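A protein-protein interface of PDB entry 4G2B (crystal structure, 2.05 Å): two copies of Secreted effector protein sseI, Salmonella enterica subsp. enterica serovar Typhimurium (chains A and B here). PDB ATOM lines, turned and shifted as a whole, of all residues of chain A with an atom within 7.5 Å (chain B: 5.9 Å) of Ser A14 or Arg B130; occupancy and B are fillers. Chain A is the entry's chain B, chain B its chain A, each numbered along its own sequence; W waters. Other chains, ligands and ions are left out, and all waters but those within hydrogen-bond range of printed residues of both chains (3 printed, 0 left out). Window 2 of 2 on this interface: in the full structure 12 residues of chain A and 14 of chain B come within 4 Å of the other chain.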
ATOM      1  N   TYR A  10      21.230  19.257  38.086  1.00  0.00           N
ATOM      2  CA  TYR A  10      20.291  18.282  37.477  1.00  0.00           C
ATOM      3  C   TYR A  10      20.516  16.836  37.924  1.00  0.00           C
ATOM      4  O   TYR A  10      21.615  16.475  38.355  1.00  0.00           O
ATOM      5  CB  TYR A  10      20.291  18.382  35.980  1.00  0.00           C
ATOM      6  CG  TYR A  10      21.523  17.889  35.264  1.00  0.00           C
ATOM      7  CD1 TYR A  10      22.500  18.778  34.834  1.00  0.00           C
ATOM      8  CD2 TYR A  10      21.687  16.540  34.965  1.00  0.00           C
ATOM      9  CE1 TYR A  10      23.563  18.376  34.153  1.00  0.00           C
ATOM     10  CE2 TYR A  10      22.792  16.104  34.261  1.00  0.00           C
ATOM     11  CZ  TYR A  10      23.729  17.056  33.852  1.00  0.00           C
ATOM     12  OH  TYR A  10      24.822  16.671  33.153  1.00  0.00           O
ATOM     13  N   LEU A  12      18.928  13.895  36.336  1.00  0.00           N
ATOM     14  CA  LEU A  12      18.685  12.981  35.285  1.00  0.00           C
ATOM     15  C   LEU A  12      19.450  13.414  34.071  1.00  0.00           C
ATOM     16  O   LEU A  12      19.286  14.543  33.613  1.00  0.00           O
ATOM     17  CB  LEU A  12      17.182  12.913  34.954  1.00  0.00           C
ATOM     18  CG  LEU A  12      16.265  12.575  36.130  1.00  0.00           C
ATOM     19  CD1 LEU A  12      14.770  12.750  35.766  1.00  0.00           C
ATOM     20  CD2 LEU A  12      16.557  11.201  36.732  1.00  0.00           C
ATOM     21  N   THR A  13      20.268  12.523  33.535  1.00  0.00           N
ATOM     22  CA  THR A  13      21.064  12.795  32.329  1.00  0.00           C
ATOM     23  C   THR A  13      20.126  12.886  31.093  1.00  0.00           C
ATOM     24  O   THR A  13      19.003  12.359  31.152  1.00  0.00           O
ATOM     25  CB  THR A  13      22.156  11.675  32.134  1.00  0.00           C
ATOM     26  OG1 THR A  13      23.060  12.051  31.087  1.00  0.00           O
ATOM     27  CG2 THR A  13      21.535  10.230  31.818  1.00  0.00           C
ATOM     28  N   SER A  14      20.572  13.555  30.016  1.00  0.00           N
ATOM     29  CA  SER A  14      19.935  13.493  28.678  1.00  0.00           C
ATOM     30  C   SER A  14      20.839  12.711  27.748  1.00  0.00           C
ATOM     31  O   SER A  14      20.559  12.608  26.539  1.00  0.00           O
ATOM     32  CB  SER A  14      19.685  14.873  28.029  1.00  0.00           C
ATOM     33  OG  SER A  14      19.976  15.939  28.914  1.00  0.00           O
ATOM     34  N   ASP A  15      21.923  12.141  28.274  1.00  0.00           N
ATOM     35  CA  ASP A  15      22.687  11.184  27.457  1.00  0.00           C
ATOM     36  C   ASP A  15      21.807  10.000  27.073  1.00  0.00           C
ATOM     37  O   ASP A  15      21.895   9.466  25.945  1.00  0.00           O
ATOM     38  CB  ASP A  15      23.870  10.618  28.219  1.00  0.00           C
ATOM     39  CG  ASP A  15      25.056  11.535  28.265  1.00  0.00           C
ATOM     40  OD1 ASP A  15      24.982  12.672  27.727  1.00  0.00           O
ATOM     41  OD2 ASP A  15      26.087  11.107  28.894  1.00  0.00           O
ATOM     42  N   ILE A  16      20.983   9.562  28.026  1.00  0.00           N
ATOM     43  CA  ILE A  16      19.951   8.518  27.815  1.00  0.00           C
ATOM     44  C   ILE A  16      18.669   9.141  28.234  1.00  0.00           C
ATOM     45  O   ILE A  16      18.665  10.186  28.879  1.00  0.00           O
ATOM     46  CB  ILE A  16      20.180   7.209  28.673  1.00  0.00           C
ATOM     47  CG1 ILE A  16      20.356   7.489  30.170  1.00  0.00           C
ATOM     48  CG2 ILE A  16      21.345   6.459  28.161  1.00  0.00           C
ATOM     49  CD1 ILE A  16      20.748   6.195  30.959  1.00  0.00           C
ATOM     50  N   ASP A  17      17.560   8.515  27.925  1.00  0.00           N
ATOM     51  CA  ASP A  17      16.287   9.034  28.417  1.00  0.00           C
ATOM     52  C   ASP A  17      15.927   8.656  29.894  1.00  0.00           C
ATOM     53  O   ASP A  17      14.997   7.892  30.180  1.00  0.00           O
ATOM     54  CB  ASP A  17      15.181   8.639  27.493  1.00  0.00           C
ATOM     55  CG  ASP A  17      13.941   9.452  27.724  1.00  0.00           C
ATOM     56  OD1 ASP A  17      13.923  10.354  28.607  1.00  0.00           O
ATOM     57  OD2 ASP A  17      12.970   9.171  26.990  1.00  0.00           O
ATOM     58  N   ALA A  18      16.686   9.246  30.805  1.00  0.00           N
ATOM     59  CA  ALA A  18      16.542   9.055  32.235  1.00  0.00           C
ATOM     60  C   ALA A  18      15.187   9.508  32.770  1.00  0.00           C
ATOM     61  O   ALA A  18      14.642   8.882  33.674  1.00  0.00           O
ATOM     62  CB  ALA A  18      17.597   9.813  32.910  1.00  0.00           C
ATOM     63  N   ALA A  19      14.667  10.625  32.238  1.00  0.00           N
ATOM     64  CA  ALA A  19      13.315  11.126  32.559  1.00  0.00           C
ATOM     65  C   ALA A  19      12.220  10.035  32.400  1.00  0.00           C
ATOM     66  O   ALA A  19      11.395   9.811  33.287  1.00  0.00           O
ATOM     67  CB  ALA A  19      12.982  12.315  31.650  1.00  0.00           C
ATOM     68  N   TYR A  92      26.404   4.220  33.080  1.00  0.00           N
ATOM     69  CA  TYR A  92      25.343   5.006  33.732  1.00  0.00           C
ATOM     70  C   TYR A  92      25.061   4.458  35.130  1.00  0.00           C
ATOM     71  O   TYR A  92      25.135   3.259  35.326  1.00  0.00           O
ATOM     72  CB  TYR A  92      24.052   4.927  32.906  1.00  0.00           C
ATOM     73  CG  TYR A  92      24.298   5.576  31.575  1.00  0.00           C
ATOM     74  CD1 TYR A  92      24.229   6.935  31.458  1.00  0.00           C
ATOM     75  CD2 TYR A  92      24.698   4.842  30.486  1.00  0.00           C
ATOM     76  CE1 TYR A  92      24.506   7.568  30.222  1.00  0.00           C
ATOM     77  CE2 TYR A  92      24.959   5.458  29.235  1.00  0.00           C
ATOM     78  CZ  TYR A  92      24.877   6.821  29.147  1.00  0.00           C
ATOM     79  OH  TYR A  92      25.122   7.480  27.991  1.00  0.00           O
ATOM     80  N   ILE A 114      19.666   9.443  37.927  1.00  0.00           N
ATOM     81  CA  ILE A 114      20.056   8.527  36.825  1.00  0.00           C
ATOM     82  C   ILE A 114      21.014   9.322  35.985  1.00  0.00           C
ATOM     83  O   ILE A 114      20.612  10.150  35.218  1.00  0.00           O
ATOM     84  CB  ILE A 114      18.839   8.052  35.951  1.00  0.00           C
ATOM     85  CG1 ILE A 114      17.857   7.312  36.832  1.00  0.00           C
ATOM     86  CG2 ILE A 114      19.248   7.143  34.821  1.00  0.00           C
ATOM     87  CD1 ILE A 114      16.527   7.057  36.095  1.00  0.00           C
ATOM     88  N   LEU A 115      22.291   9.022  36.090  1.00  0.00           N
ATOM     89  CA  LEU A 115      23.314   9.877  35.529  1.00  0.00           C
ATOM     90  C   LEU A 115      24.368   9.020  34.803  1.00  0.00           C
ATOM     91  O   LEU A 115      24.574   7.823  35.128  1.00  0.00           O
ATOM     92  CB  LEU A 115      23.863  10.693  36.683  1.00  0.00           C
ATOM     93  CG  LEU A 115      23.015  11.827  37.291  1.00  0.00           C
ATOM     94  CD1 LEU A 115      23.750  12.384  38.652  1.00  0.00           C
ATOM     95  CD2 LEU A 115      22.674  12.968  36.264  1.00  0.00           C
ATOM     96  N   SER A 116      25.074   9.623  33.839  1.00  0.00           N
ATOM     97  CA  SER A 116      26.367   9.069  33.386  1.00  0.00           C
ATOM     98  C   SER A 116      27.348   8.898  34.599  1.00  0.00           C
ATOM     99  O   SER A 116      27.218   9.554  35.634  1.00  0.00           O
ATOM    100  CB  SER A 116      27.035   9.962  32.314  1.00  0.00           C
ATOM    101  OG  SER A 116      27.640  11.076  32.985  1.00  0.00           O
ATOM    102  N   GLU A 119      28.850  12.161  35.553  1.00  0.00           N
ATOM    103  CA  GLU A 119      27.945  13.080  36.207  1.00  0.00           C
ATOM    104  C   GLU A 119      27.655  12.703  37.648  1.00  0.00           C
ATOM    105  O   GLU A 119      27.451  13.561  38.516  1.00  0.00           O
ATOM    106  CB  GLU A 119      26.645  13.210  35.429  1.00  0.00           C
ATOM    107  CG  GLU A 119      26.768  13.845  34.107  1.00  0.00           C
ATOM    108  CD  GLU A 119      25.626  13.461  33.134  1.00  0.00           C
ATOM    109  OE1 GLU A 119      25.147  12.341  33.102  1.00  0.00           O
ATOM    110  OE2 GLU A 119      25.291  14.272  32.313  1.00  0.00           O
ATOM    111  N   TRP B  69      28.748  26.141  23.432  1.00  0.00           N
ATOM    112  CA  TRP B  69      27.898  26.036  22.250  1.00  0.00           C
ATOM    113  C   TRP B  69      26.473  25.610  22.667  1.00  0.00           C
ATOM    114  O   TRP B  69      26.286  24.648  23.444  1.00  0.00           O
ATOM    115  CB  TRP B  69      28.459  24.997  21.251  1.00  0.00           C
ATOM    116  CG  TRP B  69      29.752  25.385  20.564  1.00  0.00           C
ATOM    117  CD1 TRP B  69      31.027  25.133  21.002  1.00  0.00           C
ATOM    118  CD2 TRP B  69      29.890  26.098  19.330  1.00  0.00           C
ATOM    119  NE1 TRP B  69      31.946  25.641  20.113  1.00  0.00           N
ATOM    120  CE2 TRP B  69      31.273  26.229  19.069  1.00  0.00           C
ATOM    121  CE3 TRP B  69      28.979  26.641  18.419  1.00  0.00           C
ATOM    122  CZ2 TRP B  69      31.755  26.865  17.946  1.00  0.00           C
ATOM    123  CZ3 TRP B  69      29.474  27.305  17.289  1.00  0.00           C
ATOM    124  CH2 TRP B  69      30.846  27.397  17.060  1.00  0.00           C
ATOM    125  N   ASP B  70      25.481  26.343  22.155  1.00  0.00           N
ATOM    126  CA  ASP B  70      24.072  26.038  22.453  1.00  0.00           C
ATOM    127  C   ASP B  70      23.505  25.063  21.478  1.00  0.00           C
ATOM    128  O   ASP B  70      22.661  24.267  21.837  1.00  0.00           O
ATOM    129  CB  ASP B  70      23.247  27.303  22.449  1.00  0.00           C
ATOM    130  CG  ASP B  70      23.619  28.200  23.579  1.00  0.00           C
ATOM    131  OD1 ASP B  70      23.551  27.734  24.715  1.00  0.00           O
ATOM    132  OD2 ASP B  70      24.017  29.374  23.371  1.00  0.00           O
ATOM    133  N   THR B 128      24.819  22.659  33.179  1.00  0.00           N
ATOM    134  CA  THR B 128      24.022  22.641  31.973  1.00  0.00           C
ATOM    135  C   THR B 128      23.714  21.214  31.560  1.00  0.00           C
ATOM    136  O   THR B 128      24.511  20.304  31.715  1.00  0.00           O
ATOM    137  CB  THR B 128      24.669  23.458  30.799  1.00  0.00           C
ATOM    138  OG1 THR B 128      23.870  23.331  29.608  1.00  0.00           O
ATOM    139  CG2 THR B 128      26.093  22.999  30.522  1.00  0.00           C
ATOM    140  N   ARG B 129      22.551  21.069  30.950  1.00  0.00           N
ATOM    141  CA  ARG B 129      22.028  19.808  30.553  1.00  0.00           C
ATOM    142  C   ARG B 129      22.437  19.623  29.113  1.00  0.00           C
ATOM    143  O   ARG B 129      22.725  18.525  28.705  1.00  0.00           O
ATOM    144  CB  ARG B 129      20.466  19.766  30.664  1.00  0.00           C
ATOM    145  CG  ARG B 129      19.748  20.827  31.583  1.00  0.00           C
ATOM    146  CD  ARG B 129      20.104  22.362  31.350  1.00  0.00           C
ATOM    147  NE  ARG B 129      20.128  22.749  29.942  1.00  0.00           N
ATOM    148  CZ  ARG B 129      20.770  23.795  29.424  1.00  0.00           C
ATOM    149  NH1 ARG B 129      21.553  24.591  30.144  1.00  0.00           N
ATOM    150  NH2 ARG B 129      20.667  24.019  28.131  1.00  0.00           N
ATOM    151  N   ARG B 130      22.416  20.664  28.301  1.00  0.00           N
ATOM    152  CA  ARG B 130      22.630  20.453  26.902  1.00  0.00           C
ATOM    153  C   ARG B 130      23.583  21.418  26.188  1.00  0.00           C
ATOM    154  O   ARG B 130      23.609  21.418  24.955  1.00  0.00           O
ATOM    155  CB  ARG B 130      21.281  20.401  26.152  1.00  0.00           C
ATOM    156  CG  ARG B 130      20.259  21.517  26.496  1.00  0.00           C
ATOM    157  CD  ARG B 130      18.787  21.239  25.987  1.00  0.00           C
ATOM    158  NE  ARG B 130      18.430  19.804  25.973  1.00  0.00           N
ATOM    159  CZ  ARG B 130      18.157  19.058  27.053  1.00  0.00           C
ATOM    160  NH1 ARG B 130      18.163  19.602  28.279  1.00  0.00           N
ATOM    161  NH2 ARG B 130      17.853  17.760  26.905  1.00  0.00           N
ATOM    162  N   LYS B 131      24.357  22.227  26.902  1.00  0.00           N
ATOM    163  CA  LYS B 131      25.377  23.004  26.186  1.00  0.00           C
ATOM    164  C   LYS B 131      26.652  22.129  26.052  1.00  0.00           C
ATOM    165  O   LYS B 131      26.961  21.327  26.930  1.00  0.00           O
ATOM    166  CB  LYS B 131      25.663  24.335  26.854  1.00  0.00           C
ATOM    167  CG  LYS B 131      24.538  25.383  26.668  1.00  0.00           C
ATOM    168  CD  LYS B 131      24.548  26.372  27.787  1.00  0.00           C
ATOM    169  CE  LYS B 131      23.387  27.385  27.768  1.00  0.00           C
ATOM    170  NZ  LYS B 131      23.866  28.734  27.511  1.00  0.00           N
ATOM    171  N   LEU B 132      27.302  22.271  24.899  1.00  0.00           N
ATOM    172  CA  LEU B 132      28.612  21.746  24.621  1.00  0.00           C
ATOM    173  C   LEU B 132      29.671  22.701  25.159  1.00  0.00           C
ATOM    174  O   LEU B 132      29.680  23.888  24.821  1.00  0.00           O
ATOM    175  CB  LEU B 132      28.787  21.625  23.135  1.00  0.00           C
ATOM    176  CG  LEU B 132      30.178  21.234  22.654  1.00  0.00           C
ATOM    177  CD1 LEU B 132      30.704  19.858  23.246  1.00  0.00           C
ATOM    178  CD2 LEU B 132      30.164  21.187  21.120  1.00  0.00           C
ATOM    179  N   THR B 167      31.608  18.949  28.657  1.00  0.00           N
ATOM    180  CA  THR B 167      30.375  18.224  28.300  1.00  0.00           C
ATOM    181  C   THR B 167      30.511  17.677  26.920  1.00  0.00           C
ATOM    182  O   THR B 167      31.435  18.029  26.209  1.00  0.00           O
ATOM    183  CB  THR B 167      29.143  19.065  28.367  1.00  0.00           C
ATOM    184  OG1 THR B 167      29.130  20.033  27.302  1.00  0.00           O
ATOM    185  CG2 THR B 167      29.051  19.754  29.715  1.00  0.00           C
ATOM    186  N   PRO B 169      27.238  16.617  24.930  1.00  0.00           N
ATOM    187  CA  PRO B 169      25.854  16.265  24.957  1.00  0.00           C
ATOM    188  C   PRO B 169      25.452  15.424  23.772  1.00  0.00           C
ATOM    189  O   PRO B 169      26.127  15.394  22.729  1.00  0.00           O
ATOM    190  CB  PRO B 169      25.125  17.603  24.943  1.00  0.00           C
ATOM    191  CG  PRO B 169      26.157  18.621  24.373  1.00  0.00           C
ATOM    192  CD  PRO B 169      27.497  18.002  24.511  1.00  0.00           C
ATOM    193  N   ARG B 170      24.334  14.723  23.977  1.00  0.00           N
ATOM    194  CA  ARG B 170      23.801  13.769  23.003  1.00  0.00           C
ATOM    195  C   ARG B 170      23.798  14.323  21.550  1.00  0.00           C
ATOM    196  O   ARG B 170      24.369  13.688  20.609  1.00  0.00           O
ATOM    197  CB  ARG B 170      22.390  13.336  23.434  1.00  0.00           C
ATOM    198  CG  ARG B 170      21.877  12.209  22.669  1.00  0.00           C
ATOM    199  CD  ARG B 170      20.485  11.848  23.166  1.00  0.00           C
ATOM    200  NE  ARG B 170      20.373  10.401  23.347  1.00  0.00           N
ATOM    201  CZ  ARG B 170      19.236   9.762  23.631  1.00  0.00           C
ATOM    202  NH1 ARG B 170      18.082  10.440  23.778  1.00  0.00           N
ATOM    203  NH2 ARG B 170      19.251   8.435  23.783  1.00  0.00           N
ATOM    204  N   TRP B 171      23.228  15.513  21.409  1.00  0.00           N
ATOM    205  CA  TRP B 171      23.166  16.229  20.114  1.00  0.00           C
ATOM    206  C   TRP B 171      24.524  16.487  19.433  1.00  0.00           C
ATOM    207  O   TRP B 171      24.632  16.515  18.184  1.00  0.00           O
ATOM    208  CB  TRP B 171      22.440  17.564  20.250  1.00  0.00           C
ATOM    209  CG  TRP B 171      23.181  18.709  20.959  1.00  0.00           C
ATOM    210  CD1 TRP B 171      22.917  19.168  22.216  1.00  0.00           C
ATOM    211  CD2 TRP B 171      24.207  19.595  20.424  1.00  0.00           C
ATOM    212  NE1 TRP B 171      23.722  20.253  22.518  1.00  0.00           N
ATOM    213  CE2 TRP B 171      24.536  20.524  21.450  1.00  0.00           C
ATOM    214  CE3 TRP B 171      24.907  19.665  19.210  1.00  0.00           C
ATOM    215  CZ2 TRP B 171      25.504  21.536  21.282  1.00  0.00           C
ATOM    216  CZ3 TRP B 171      25.898  20.660  19.052  1.00  0.00           C
ATOM    217  CH2 TRP B 171      26.189  21.575  20.088  1.00  0.00           C
HETATM  218  O   HOH W   1      23.396  14.508  26.654  1.00  0.00           O
HETATM  219  O   HOH W   2      26.449  18.185  31.407  1.00  0.00           O
HETATM  220  O   HOH W   3      17.719  11.912  26.201  1.00  0.00           O
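Printed residues of chain B within 4 Å of Tyr A10: Thr B128.
Ser A14 touches just these residues of chain B: Arg B129, Arg B130 and Arg B170.
Of the printed residues of chain B, Asp A15 touches Arg B170 (3.2 Å).
Ile A16 touches none of the printed residues of chain B.
Of chain A, only Ser A14 (3.4 Å) comes within 4 Å of Arg B130.
Printed residues of chain A within 4 Å of Arg B170: Ser A14 (3.5 Å) and Asp A15 (3.2 Å).
The nearest printed residue of chain B that does not touch Tyr A10 is Arg B129 (4.2 Å).
No position is printed for both chains.
Of the 5 pairs that touch across the chains among the printed residues, none has its exchanged pair printed and touching as well.
The guanidinium group of Arg B130 is in hydrogen-bond range of the side-chain hydroxyl of Ser A14, at 3.4 Å.
The guanidinium group (NE) of Arg B170 sits at hydrogen-bond distance from the backbone carbonyl oxygen (O) of Asp A15 (3.2 Å).
OG1 of Thr B128 is in hydrogen-bond range of NH1 of Arg B129 (2.7 Å).
OG1 of Thr B128 sits at hydrogen-bond distance from N of Arg B130 (3.3 Å).
OG1 of Thr B128 sits at hydrogen-bond distance from N of Lys B131 (3.0 Å).
The indole nitrogen (NE1) of Trp B171 lies within hydrogen-bond range of the backbone carbonyl oxygen (O) of Arg B130.
OH of Tyr A10 sits at hydrogen-bond distance from OE2 of Glu A119 (2.6 Å).
The side-chain hydroxyl (OG1) of Thr A13 lies within hydrogen-bond range of the backbone NH (N) of Asp A15.
Among the printed residues, merely in contact across the chains: Tyr A10 with Thr B128, Ser A14 with Arg B170 and Ser A14 with Arg B129.
Water W1 lies within hydrogen-bond range of the side-chain carboxylate of Asp A15 (2.7 Å), the backbone NH of Arg B170 (2.8 Å) and the backbone carbonyl oxygen of Ser A14 (3.4 Å).
Water W2 bridges the side-chain hydroxyl of Tyr A10 (2.8 Å) and the backbone carbonyl oxygen of Thr B128 (2.9 Å).
Water W3 lies within hydrogen-bond range of NH1 of Arg B170 (2.9 Å), O of Ser A14 (2.9 Å) and O of Ile A16 (3.3 Å).
Of the 14 printed residues of chain A, 3 touch a printed residue of chain B.
Printed residues of chain A that touch a printed residue of chain B: Tyr A10, Ser A14 and Asp A15.
Of the 11 printed residues of chain B, 4 touch a printed residue of chain A.
Among the printed residues, no Asp or Glu carboxylate lies within 4 Å of a Lys or Arg side-chain nitrogen of the other chain.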
